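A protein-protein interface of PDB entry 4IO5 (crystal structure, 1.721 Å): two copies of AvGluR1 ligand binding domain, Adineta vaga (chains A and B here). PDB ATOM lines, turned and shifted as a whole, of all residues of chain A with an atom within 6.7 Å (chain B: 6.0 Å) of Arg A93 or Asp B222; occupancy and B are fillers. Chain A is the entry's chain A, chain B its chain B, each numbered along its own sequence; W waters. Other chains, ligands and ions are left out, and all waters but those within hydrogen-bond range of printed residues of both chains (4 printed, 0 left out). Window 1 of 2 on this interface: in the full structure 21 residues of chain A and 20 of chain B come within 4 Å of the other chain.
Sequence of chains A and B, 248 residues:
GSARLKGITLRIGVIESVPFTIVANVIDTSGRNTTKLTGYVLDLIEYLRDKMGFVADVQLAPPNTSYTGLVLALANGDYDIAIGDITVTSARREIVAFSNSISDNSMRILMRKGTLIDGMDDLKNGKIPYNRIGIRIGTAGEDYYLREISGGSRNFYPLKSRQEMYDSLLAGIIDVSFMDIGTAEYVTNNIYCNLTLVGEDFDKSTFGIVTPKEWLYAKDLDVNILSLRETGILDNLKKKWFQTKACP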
ATOM      1  N   VAL A  71       6.216  25.320  26.285  1.00  0.00           N
ATOM      2  CA  VAL A  71       5.897  25.292  24.865  1.00  0.00           C
ATOM      3  C   VAL A  71       6.045  26.681  24.203  1.00  0.00           C
ATOM      4  O   VAL A  71       6.656  26.815  23.154  1.00  0.00           O
ATOM      5  CB  VAL A  71       4.491  24.729  24.677  1.00  0.00           C
ATOM      6  CG1 VAL A  71       4.007  24.890  23.281  1.00  0.00           C
ATOM      7  CG2 VAL A  71       4.483  23.268  25.062  1.00  0.00           C
ATOM      8  N   VAL A  88       0.621  16.200  24.171  1.00  0.00           N
ATOM      9  CA  VAL A  88       0.370  16.703  22.832  1.00  0.00           C
ATOM     10  C   VAL A  88      -1.080  17.160  22.794  1.00  0.00           C
ATOM     11  O   VAL A  88      -1.999  16.357  22.995  1.00  0.00           O
ATOM     12  CB  VAL A  88       0.641  15.607  21.771  1.00  0.00           C
ATOM     13  CG1 VAL A  88       0.390  16.167  20.354  1.00  0.00           C
ATOM     14  CG2 VAL A  88       2.044  15.068  21.895  1.00  0.00           C
ATOM     15  N   THR A  89      -1.316  18.438  22.530  1.00  0.00           N
ATOM     16  CA  THR A  89      -2.673  18.955  22.467  1.00  0.00           C
ATOM     17  C   THR A  89      -2.887  19.739  21.174  1.00  0.00           C
ATOM     18  O   THR A  89      -1.944  20.225  20.574  1.00  0.00           O
ATOM     19  CB  THR A  89      -2.981  19.892  23.660  1.00  0.00           C
ATOM     20  OG1 THR A  89      -2.300  21.136  23.471  1.00  0.00           O
ATOM     21  CG2 THR A  89      -2.551  19.231  25.012  1.00  0.00           C
ATOM     22  N   SER A  90      -4.135  19.868  20.762  1.00  0.00           N
ATOM     23  CA  SER A  90      -4.467  20.598  19.538  1.00  0.00           C
ATOM     24  C   SER A  90      -4.036  22.061  19.619  1.00  0.00           C
ATOM     25  O   SER A  90      -3.474  22.613  18.679  1.00  0.00           O
ATOM     26  CB  SER A  90      -5.970  20.497  19.292  1.00  0.00           C
ATOM     27  OG  SER A  90      -6.318  20.986  18.010  1.00  0.00           O
ATOM     28  N   ALA A  91      -4.301  22.690  20.759  1.00  0.00           N
ATOM     29  CA  ALA A  91      -3.896  24.075  20.956  1.00  0.00           C
ATOM     30  C   ALA A  91      -2.366  24.253  20.869  1.00  0.00           C
ATOM     31  O   ALA A  91      -1.876  25.239  20.264  1.00  0.00           O
ATOM     32  CB  ALA A  91      -4.412  24.564  22.273  1.00  0.00           C
ATOM     33  N   ARG A  92      -1.593  23.313  21.425  1.00  0.00           N
ATOM     34  CA  ARG A  92      -0.144  23.456  21.359  1.00  0.00           C
ATOM     35  C   ARG A  92       0.371  23.186  19.943  1.00  0.00           C
ATOM     36  O   ARG A  92       1.302  23.823  19.474  1.00  0.00           O
ATOM     37  CB  ARG A  92       0.538  22.540  22.371  1.00  0.00           C
ATOM     38  CG  ARG A  92       0.321  22.948  23.788  1.00  0.00           C
ATOM     39  CD  ARG A  92       0.674  21.804  24.772  1.00  0.00           C
ATOM     40  NE  ARG A  92       0.413  22.250  26.131  1.00  0.00           N
ATOM     41  CZ  ARG A  92       0.641  21.512  27.200  1.00  0.00           C
ATOM     42  NH1 ARG A  92       1.106  20.284  27.070  1.00  0.00           N
ATOM     43  NH2 ARG A  92       0.396  22.008  28.402  1.00  0.00           N
ATOM     44  N   ARG A  93      -0.276  22.257  19.247  1.00  0.00           N
ATOM     45  CA  ARG A  93       0.132  21.883  17.891  1.00  0.00           C
ATOM     46  C   ARG A  93      -0.061  23.040  16.893  1.00  0.00           C
ATOM     47  O   ARG A  93       0.592  23.093  15.861  1.00  0.00           O
ATOM     48  CB  ARG A  93      -0.672  20.673  17.434  1.00  0.00           C
ATOM     49  CG  ARG A  93      -0.288  20.184  16.036  1.00  0.00           C
ATOM     50  CD  ARG A  93       1.098  19.553  16.015  1.00  0.00           C
ATOM     51  NE  ARG A  93       1.522  19.236  14.653  1.00  0.00           N
ATOM     52  CZ  ARG A  93       2.026  20.103  13.775  1.00  0.00           C
ATOM     53  NH1 ARG A  93       2.264  21.367  14.106  1.00  0.00           N
ATOM     54  NH2 ARG A  93       2.381  19.672  12.553  1.00  0.00           N
ATOM     55  N   GLU A  94      -0.915  24.005  17.232  1.00  0.00           N
ATOM     56  CA  GLU A  94      -1.031  25.228  16.434  1.00  0.00           C
ATOM     57  C   GLU A  94       0.271  26.019  16.385  1.00  0.00           C
ATOM     58  O   GLU A  94       0.519  26.683  15.389  1.00  0.00           O
ATOM     59  CB  GLU A  94      -2.154  26.137  16.958  1.00  0.00           C
ATOM     60  CG  GLU A  94      -3.544  25.577  16.804  1.00  0.00           C
ATOM     61  CD  GLU A  94      -4.131  25.737  15.386  1.00  0.00           C
ATOM     62  OE1 GLU A  94      -3.416  26.155  14.440  1.00  0.00           O
ATOM     63  OE2 GLU A  94      -5.330  25.427  15.230  1.00  0.00           O
ATOM     64  N   ILE A  95       1.107  25.940  17.432  1.00  0.00           N
ATOM     65  CA  ILE A  95       2.271  26.802  17.539  1.00  0.00           C
ATOM     66  C   ILE A  95       3.626  26.091  17.541  1.00  0.00           C
ATOM     67  O   ILE A  95       4.660  26.740  17.361  1.00  0.00           O
ATOM     68  CB  ILE A  95       2.187  27.765  18.754  1.00  0.00           C
ATOM     69  CG1 ILE A  95       2.091  26.996  20.078  1.00  0.00           C
ATOM     70  CG2 ILE A  95       1.003  28.697  18.554  1.00  0.00           C
ATOM     71  CD1 ILE A  95       2.382  27.870  21.330  1.00  0.00           C
ATOM     72  N   VAL A  96       3.605  24.784  17.764  1.00  0.00           N
ATOM     73  CA  VAL A  96       4.816  23.954  17.727  1.00  0.00           C
ATOM     74  C   VAL A  96       4.479  22.611  17.090  1.00  0.00           C
ATOM     75  O   VAL A  96       3.301  22.249  16.928  1.00  0.00           O
ATOM     76  CB  VAL A  96       5.417  23.689  19.149  1.00  0.00           C
ATOM     77  CG1 VAL A  96       5.850  24.989  19.843  1.00  0.00           C
ATOM     78  CG2 VAL A  96       4.462  22.916  20.019  1.00  0.00           C
ATOM     79  N   ALA A  97       5.504  21.867  16.713  1.00  0.00           N
ATOM     80  CA  ALA A  97       5.288  20.501  16.308  1.00  0.00           C
ATOM     81  C   ALA A  97       5.685  19.565  17.442  1.00  0.00           C
ATOM     82  O   ALA A  97       6.354  19.951  18.404  1.00  0.00           O
ATOM     83  CB  ALA A  97       6.069  20.168  15.046  1.00  0.00           C
ATOM     84  N   PHE A  98       5.278  18.309  17.295  1.00  0.00           N
ATOM     85  CA  PHE A  98       5.652  17.271  18.231  1.00  0.00           C
ATOM     86  C   PHE A  98       6.246  16.074  17.505  1.00  0.00           C
ATOM     87  O   PHE A  98       5.796  15.689  16.422  1.00  0.00           O
ATOM     88  CB  PHE A  98       4.450  16.808  19.056  1.00  0.00           C
ATOM     89  CG  PHE A  98       3.922  17.825  20.032  1.00  0.00           C
ATOM     90  CD1 PHE A  98       2.929  18.713  19.648  1.00  0.00           C
ATOM     91  CD2 PHE A  98       4.368  17.859  21.344  1.00  0.00           C
ATOM     92  CE1 PHE A  98       2.409  19.614  20.567  1.00  0.00           C
ATOM     93  CE2 PHE A  98       3.842  18.745  22.260  1.00  0.00           C
ATOM     94  CZ  PHE A  98       2.865  19.635  21.858  1.00  0.00           C
ATOM     95  N   LYS A 213       7.808  24.101  14.435  1.00  0.00           N
ATOM     96  CA  LYS A 213       7.089  23.710  13.238  1.00  0.00           C
ATOM     97  C   LYS A 213       7.996  23.643  12.018  1.00  0.00           C
ATOM     98  O   LYS A 213       8.938  24.406  11.898  1.00  0.00           O
ATOM     99  CB  LYS A 213       5.917  24.650  12.976  1.00  0.00           C
ATOM    100  CG  LYS A 213       4.860  24.595  14.079  1.00  0.00           C
ATOM    101  CD  LYS A 213       3.598  25.361  13.666  1.00  0.00           C
ATOM    102  CE  LYS A 213       3.878  26.835  13.608  1.00  0.00           C
ATOM    103  NZ  LYS A 213       2.621  27.576  13.351  1.00  0.00           N
ATOM    104  N   GLU A 214       7.680  22.716  11.125  1.00  0.00           N
ATOM    105  CA  GLU A 214       8.438  22.528   9.876  1.00  0.00           C
ATOM    106  C   GLU A 214       9.946  22.398  10.099  1.00  0.00           C
ATOM    107  O   GLU A 214      10.757  22.993   9.380  1.00  0.00           O
ATOM    108  CB  GLU A 214       8.120  23.674   8.913  1.00  0.00           C
ATOM    109  CG  GLU A 214       6.641  23.769   8.609  1.00  0.00           C
ATOM    110  CD  GLU A 214       6.259  25.077   7.950  1.00  0.00           C
ATOM    111  OE1 GLU A 214       7.137  25.746   7.383  1.00  0.00           O
ATOM    112  OE2 GLU A 214       5.077  25.444   8.011  1.00  0.00           O
ATOM    113  N   PHE B  98       3.957  10.684   9.451  1.00  0.00           N
ATOM    114  CA  PHE B  98       2.710  10.242  10.029  1.00  0.00           C
ATOM    115  C   PHE B  98       2.089  11.373  10.829  1.00  0.00           C
ATOM    116  O   PHE B  98       2.786  12.175  11.440  1.00  0.00           O
ATOM    117  CB  PHE B  98       2.931   9.084  10.990  1.00  0.00           C
ATOM    118  CG  PHE B  98       3.315   7.797  10.334  1.00  0.00           C
ATOM    119  CD1 PHE B  98       4.626   7.523  10.026  1.00  0.00           C
ATOM    120  CD2 PHE B  98       2.346   6.860  10.013  1.00  0.00           C
ATOM    121  CE1 PHE B  98       4.969   6.340   9.445  1.00  0.00           C
ATOM    122  CE2 PHE B  98       2.671   5.696   9.431  1.00  0.00           C
ATOM    123  CZ  PHE B  98       4.003   5.414   9.152  1.00  0.00           C
ATOM    124  N   SER B  99       0.774  11.400  10.837  1.00  0.00           N
ATOM    125  CA  SER B  99      -0.010  12.300  11.675  1.00  0.00           C
ATOM    126  C   SER B  99       0.142  11.936  13.126  1.00  0.00           C
ATOM    127  O   SER B  99       0.647  10.867  13.446  1.00  0.00           O
ATOM    128  CB  SER B  99      -1.480  12.193  11.321  1.00  0.00           C
ATOM    129  OG  SER B  99      -2.069  11.013  11.865  1.00  0.00           O
ATOM    130  N   ASN B 100      -0.339  12.803  14.008  1.00  0.00           N
ATOM    131  CA  ASN B 100      -0.556  12.384  15.384  1.00  0.00           C
ATOM    132  C   ASN B 100      -1.345  11.099  15.403  1.00  0.00           C
ATOM    133  O   ASN B 100      -2.179  10.848  14.535  1.00  0.00           O
ATOM    134  CB  ASN B 100      -1.293  13.461  16.170  1.00  0.00           C
ATOM    135  CG  ASN B 100      -0.386  14.620  16.487  1.00  0.00           C
ATOM    136  OD1 ASN B 100      -0.418  15.654  15.823  1.00  0.00           O
ATOM    137  ND2 ASN B 100       0.483  14.429  17.471  1.00  0.00           N
ATOM    138  N   TYR B 217       0.326  20.353   4.453  1.00  0.00           N
ATOM    139  CA  TYR B 217      -0.918  20.360   5.210  1.00  0.00           C
ATOM    140  C   TYR B 217      -0.792  19.664   6.578  1.00  0.00           C
ATOM    141  O   TYR B 217      -1.799  19.398   7.233  1.00  0.00           O
ATOM    142  CB  TYR B 217      -2.017  19.708   4.379  1.00  0.00           C
ATOM    143  CG  TYR B 217      -2.188  20.349   3.002  1.00  0.00           C
ATOM    144  CD1 TYR B 217      -2.869  21.551   2.869  1.00  0.00           C
ATOM    145  CD2 TYR B 217      -1.686  19.746   1.860  1.00  0.00           C
ATOM    146  CE1 TYR B 217      -3.040  22.137   1.631  1.00  0.00           C
ATOM    147  CE2 TYR B 217      -1.855  20.322   0.616  1.00  0.00           C
ATOM    148  CZ  TYR B 217      -2.535  21.518   0.512  1.00  0.00           C
ATOM    149  OH  TYR B 217      -2.705  22.108  -0.724  1.00  0.00           O
ATOM    150  N   ALA B 218       0.446  19.423   7.007  1.00  0.00           N
ATOM    151  CA  ALA B 218       0.733  18.639   8.233  1.00  0.00           C
ATOM    152  C   ALA B 218       0.045  19.181   9.485  1.00  0.00           C
ATOM    153  O   ALA B 218      -0.636  18.439  10.197  1.00  0.00           O
ATOM    154  CB  ALA B 218       2.250  18.535   8.465  1.00  0.00           C
ATOM    155  N   LYS B 219       0.166  20.491   9.721  1.00  0.00           N
ATOM    156  CA  LYS B 219      -0.446  21.095  10.900  1.00  0.00           C
ATOM    157  C   LYS B 219      -1.963  21.001  10.868  1.00  0.00           C
ATOM    158  O   LYS B 219      -2.588  20.650  11.879  1.00  0.00           O
ATOM    159  CB  LYS B 219      -0.022  22.568  11.031  1.00  0.00           C
ATOM    160  CG  LYS B 219      -0.524  23.237  12.306  1.00  0.00           C
ATOM    161  CD  LYS B 219      -0.315  24.753  12.275  1.00  0.00           C
ATOM    162  CE  LYS B 219      -1.267  25.412  11.278  1.00  0.00           C
ATOM    163  NZ  LYS B 219      -2.000  26.580  11.850  1.00  0.00           N
ATOM    164  N   ASP B 220      -2.573  21.334   9.728  1.00  0.00           N
ATOM    165  CA  ASP B 220      -4.030  21.324   9.629  1.00  0.00           C
ATOM    166  C   ASP B 220      -4.562  19.927   9.998  1.00  0.00           C
ATOM    167  O   ASP B 220      -5.490  19.775  10.801  1.00  0.00           O
ATOM    168  CB  ASP B 220      -4.476  21.740   8.212  1.00  0.00           C
ATOM    169  CG  ASP B 220      -5.987  22.075   8.115  1.00  0.00           C
ATOM    170  OD1 ASP B 220      -6.584  22.511   9.124  1.00  0.00           O
ATOM    171  OD2 ASP B 220      -6.585  21.926   7.015  1.00  0.00           O
ATOM    172  N   LEU B 221      -3.949  18.891   9.447  1.00  0.00           N
ATOM    173  CA  LEU B 221      -4.419  17.536   9.758  1.00  0.00           C
ATOM    174  C   LEU B 221      -4.204  17.187  11.222  1.00  0.00           C
ATOM    175  O   LEU B 221      -5.101  16.662  11.868  1.00  0.00           O
ATOM    176  CB  LEU B 221      -3.731  16.501   8.869  1.00  0.00           C
ATOM    177  CG  LEU B 221      -4.141  15.073   9.132  1.00  0.00           C
ATOM    178  CD1 LEU B 221      -5.626  14.896   8.945  1.00  0.00           C
ATOM    179  CD2 LEU B 221      -3.346  14.114   8.208  1.00  0.00           C
ATOM    180  N   ASP B 222      -3.021  17.475  11.747  1.00  0.00           N
ATOM    181  CA  ASP B 222      -2.694  17.120  13.131  1.00  0.00           C
ATOM    182  C   ASP B 222      -3.623  17.822  14.122  1.00  0.00           C
ATOM    183  O   ASP B 222      -4.119  17.211  15.064  1.00  0.00           O
ATOM    184  CB  ASP B 222      -1.251  17.502  13.477  1.00  0.00           C
ATOM    185  CG  ASP B 222      -0.220  16.472  13.043  1.00  0.00           C
ATOM    186  OD1 ASP B 222      -0.623  15.385  12.553  1.00  0.00           O
ATOM    187  OD2 ASP B 222       1.004  16.773  13.214  1.00  0.00           O
ATOM    188  N   VAL B 223      -3.861  19.108  13.919  1.00  0.00           N
ATOM    189  CA  VAL B 223      -4.741  19.846  14.841  1.00  0.00           C
ATOM    190  C   VAL B 223      -6.134  19.247  14.825  1.00  0.00           C
ATOM    191  O   VAL B 223      -6.779  19.086  15.857  1.00  0.00           O
ATOM    192  CB  VAL B 223      -4.771  21.337  14.515  1.00  0.00           C
ATOM    193  CG1 VAL B 223      -5.844  22.023  15.325  1.00  0.00           C
ATOM    194  CG2 VAL B 223      -3.390  21.967  14.790  1.00  0.00           C
ATOM    195  N   ASN B 224      -6.599  18.875  13.643  1.00  0.00           N
ATOM    196  CA  ASN B 224      -7.906  18.268  13.556  1.00  0.00           C
ATOM    197  C   ASN B 224      -7.985  16.876  14.217  1.00  0.00           C
ATOM    198  O   ASN B 224      -8.993  16.536  14.848  1.00  0.00           O
ATOM    199  CB  ASN B 224      -8.374  18.250  12.095  1.00  0.00           C
ATOM    200  CG  ASN B 224      -9.023  19.559  11.711  1.00  0.00           C
ATOM    201  OD1 ASN B 224     -10.205  19.777  11.986  1.00  0.00           O
ATOM    202  ND2 ASN B 224      -8.244  20.460  11.158  1.00  0.00           N
ATOM    203  N   ILE B 225      -6.962  16.052  14.047  1.00  0.00           N
ATOM    204  CA  ILE B 225      -6.970  14.735  14.684  1.00  0.00           C
ATOM    205  C   ILE B 225      -6.971  14.881  16.202  1.00  0.00           C
ATOM    206  O   ILE B 225      -7.680  14.187  16.923  1.00  0.00           O
ATOM    207  CB  ILE B 225      -5.734  13.941  14.282  1.00  0.00           C
ATOM    208  CG1 ILE B 225      -5.883  13.487  12.850  1.00  0.00           C
ATOM    209  CG2 ILE B 225      -5.556  12.722  15.129  1.00  0.00           C
ATOM    210  CD1 ILE B 225      -4.567  13.022  12.286  1.00  0.00           C
ATOM    211  N   LEU B 226      -6.153  15.805  16.688  1.00  0.00           N
ATOM    212  CA  LEU B 226      -6.040  15.989  18.120  1.00  0.00           C
ATOM    213  C   LEU B 226      -7.362  16.488  18.670  1.00  0.00           C
ATOM    214  O   LEU B 226      -7.759  16.120  19.776  1.00  0.00           O
ATOM    215  CB  LEU B 226      -4.886  16.944  18.444  1.00  0.00           C
ATOM    216  CG  LEU B 226      -3.491  16.339  18.265  1.00  0.00           C
ATOM    217  CD1 LEU B 226      -2.404  17.410  18.194  1.00  0.00           C
ATOM    218  CD2 LEU B 226      -3.174  15.331  19.394  1.00  0.00           C
ATOM    219  N   SER B 227      -8.058  17.316  17.893  1.00  0.00           N
ATOM    220  CA  SER B 227      -9.352  17.825  18.318  1.00  0.00           C
ATOM    221  C   SER B 227     -10.371  16.695  18.394  1.00  0.00           C
ATOM    222  O   SER B 227     -11.168  16.629  19.333  1.00  0.00           O
ATOM    223  CB  SER B 227      -9.842  18.969  17.425  1.00  0.00           C
ATOM    224  OG  SER B 227     -11.141  19.397  17.835  1.00  0.00           O
HETATM  225  O   HOH W   1       3.516  16.977  11.704  1.00  0.00           O
HETATM  226  O   HOH W   2       4.043  17.113  14.838  1.00  0.00           O
HETATM  227  O   HOH W   3      -1.557  28.465  13.825  1.00  0.00           O
HETATM  228  O   HOH W   4       2.117  16.377  16.231  1.00  0.00           O
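The guanidinium group (NH1) of Arg A93 is in hydrogen-bond range of the backbone carbonyl oxygen (O) of Val A96. N of Asn B100 sits at hydrogen-bond distance from OD1 of Asp B222. NZ of Lys A213 is in hydrogen-bond range of O of Glu A94 (3.1 Å). OG1 of Thr A89 is in hydrogen-bond range of N of Arg A92.
Water W4 lies within hydrogen-bond range of OD1 of Asn B100 (2.7 Å), OD2 of Asp B222 (3.2 Å) and NE of Arg A93 (3.3 Å). Water W2 lies within hydrogen-bond range of the backbone carbonyl oxygen of Phe A98 (2.8 Å), the guanidinium group of Arg A93 (3.3 Å) and the side-chain carboxylate of Asp B222 (3.5 Å). Water W3 lies within hydrogen-bond range of NZ of Lys B219 (2.8 Å) and OE1 of Glu A94 (3.0 Å). Water W1 lies within hydrogen-bond range of the side-chain carboxylate of Asp B222 (2.9 Å) and the guanidinium group of Arg A93 (3.0 Å).
Of the printed residues of chain B, Val A88 touches Asn B100 (3.4 Å) and Leu B226 (3.7 Å). Of the printed residues of chain B, Thr A89 touches Leu B226 (3.7 Å). Of the printed residues of chain B, Ser A90 touches Val B223 (2.9 Å) and Leu B226 (3.8 Å). Arg A93 touches five residues of chain B. Of chain A, only Arg A93 (2.9 Å) comes within 4 Å of Asp B222. Of the printed residues of chain A, Val B223 touches Ser A90 (2.9 Å), Arg A93 (3.8 Å) and Glu A94 (3.4 Å).
Among the printed residues, pairs that only touch across the chains: Val A88 with Asn B100, Glu A94 with Val B223, Arg A93 with Lys B219, Thr A89 with Leu B226, Val A88 with Leu B226, Arg A93 with Leu B226, Arg A93 with Val B223, Ser A90 with Leu B226 and Arg A93 with Ala B218.
Of the 14 printed residues of chain A, 5 touch a printed residue of chain B. Hydrophobic or aromatic side chains of chain A within 4 Å of the printed part of chain B: Val A88. Along chain B the printed residues that touch a printed residue of chain A span positions 100 to 226.
Position printed for both chains: 98. Of the 12 pairs that touch across the chains among the printed residues, none has its exchanged pair printed and touching as well.
NZ of Lys B219 lies within salt-bridge range of OE1 of Glu A94, 3.0 Å away. The side-chain hydroxyl (OG) of Ser A90 sits at hydrogen-bond distance from the backbone carbonyl oxygen (O) of Val B223, at 2.9 Å. The side-chain carboxylate (OD2) of Asp B222 lies within salt-bridge range of the guanidinium group (NE) of Arg A93.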
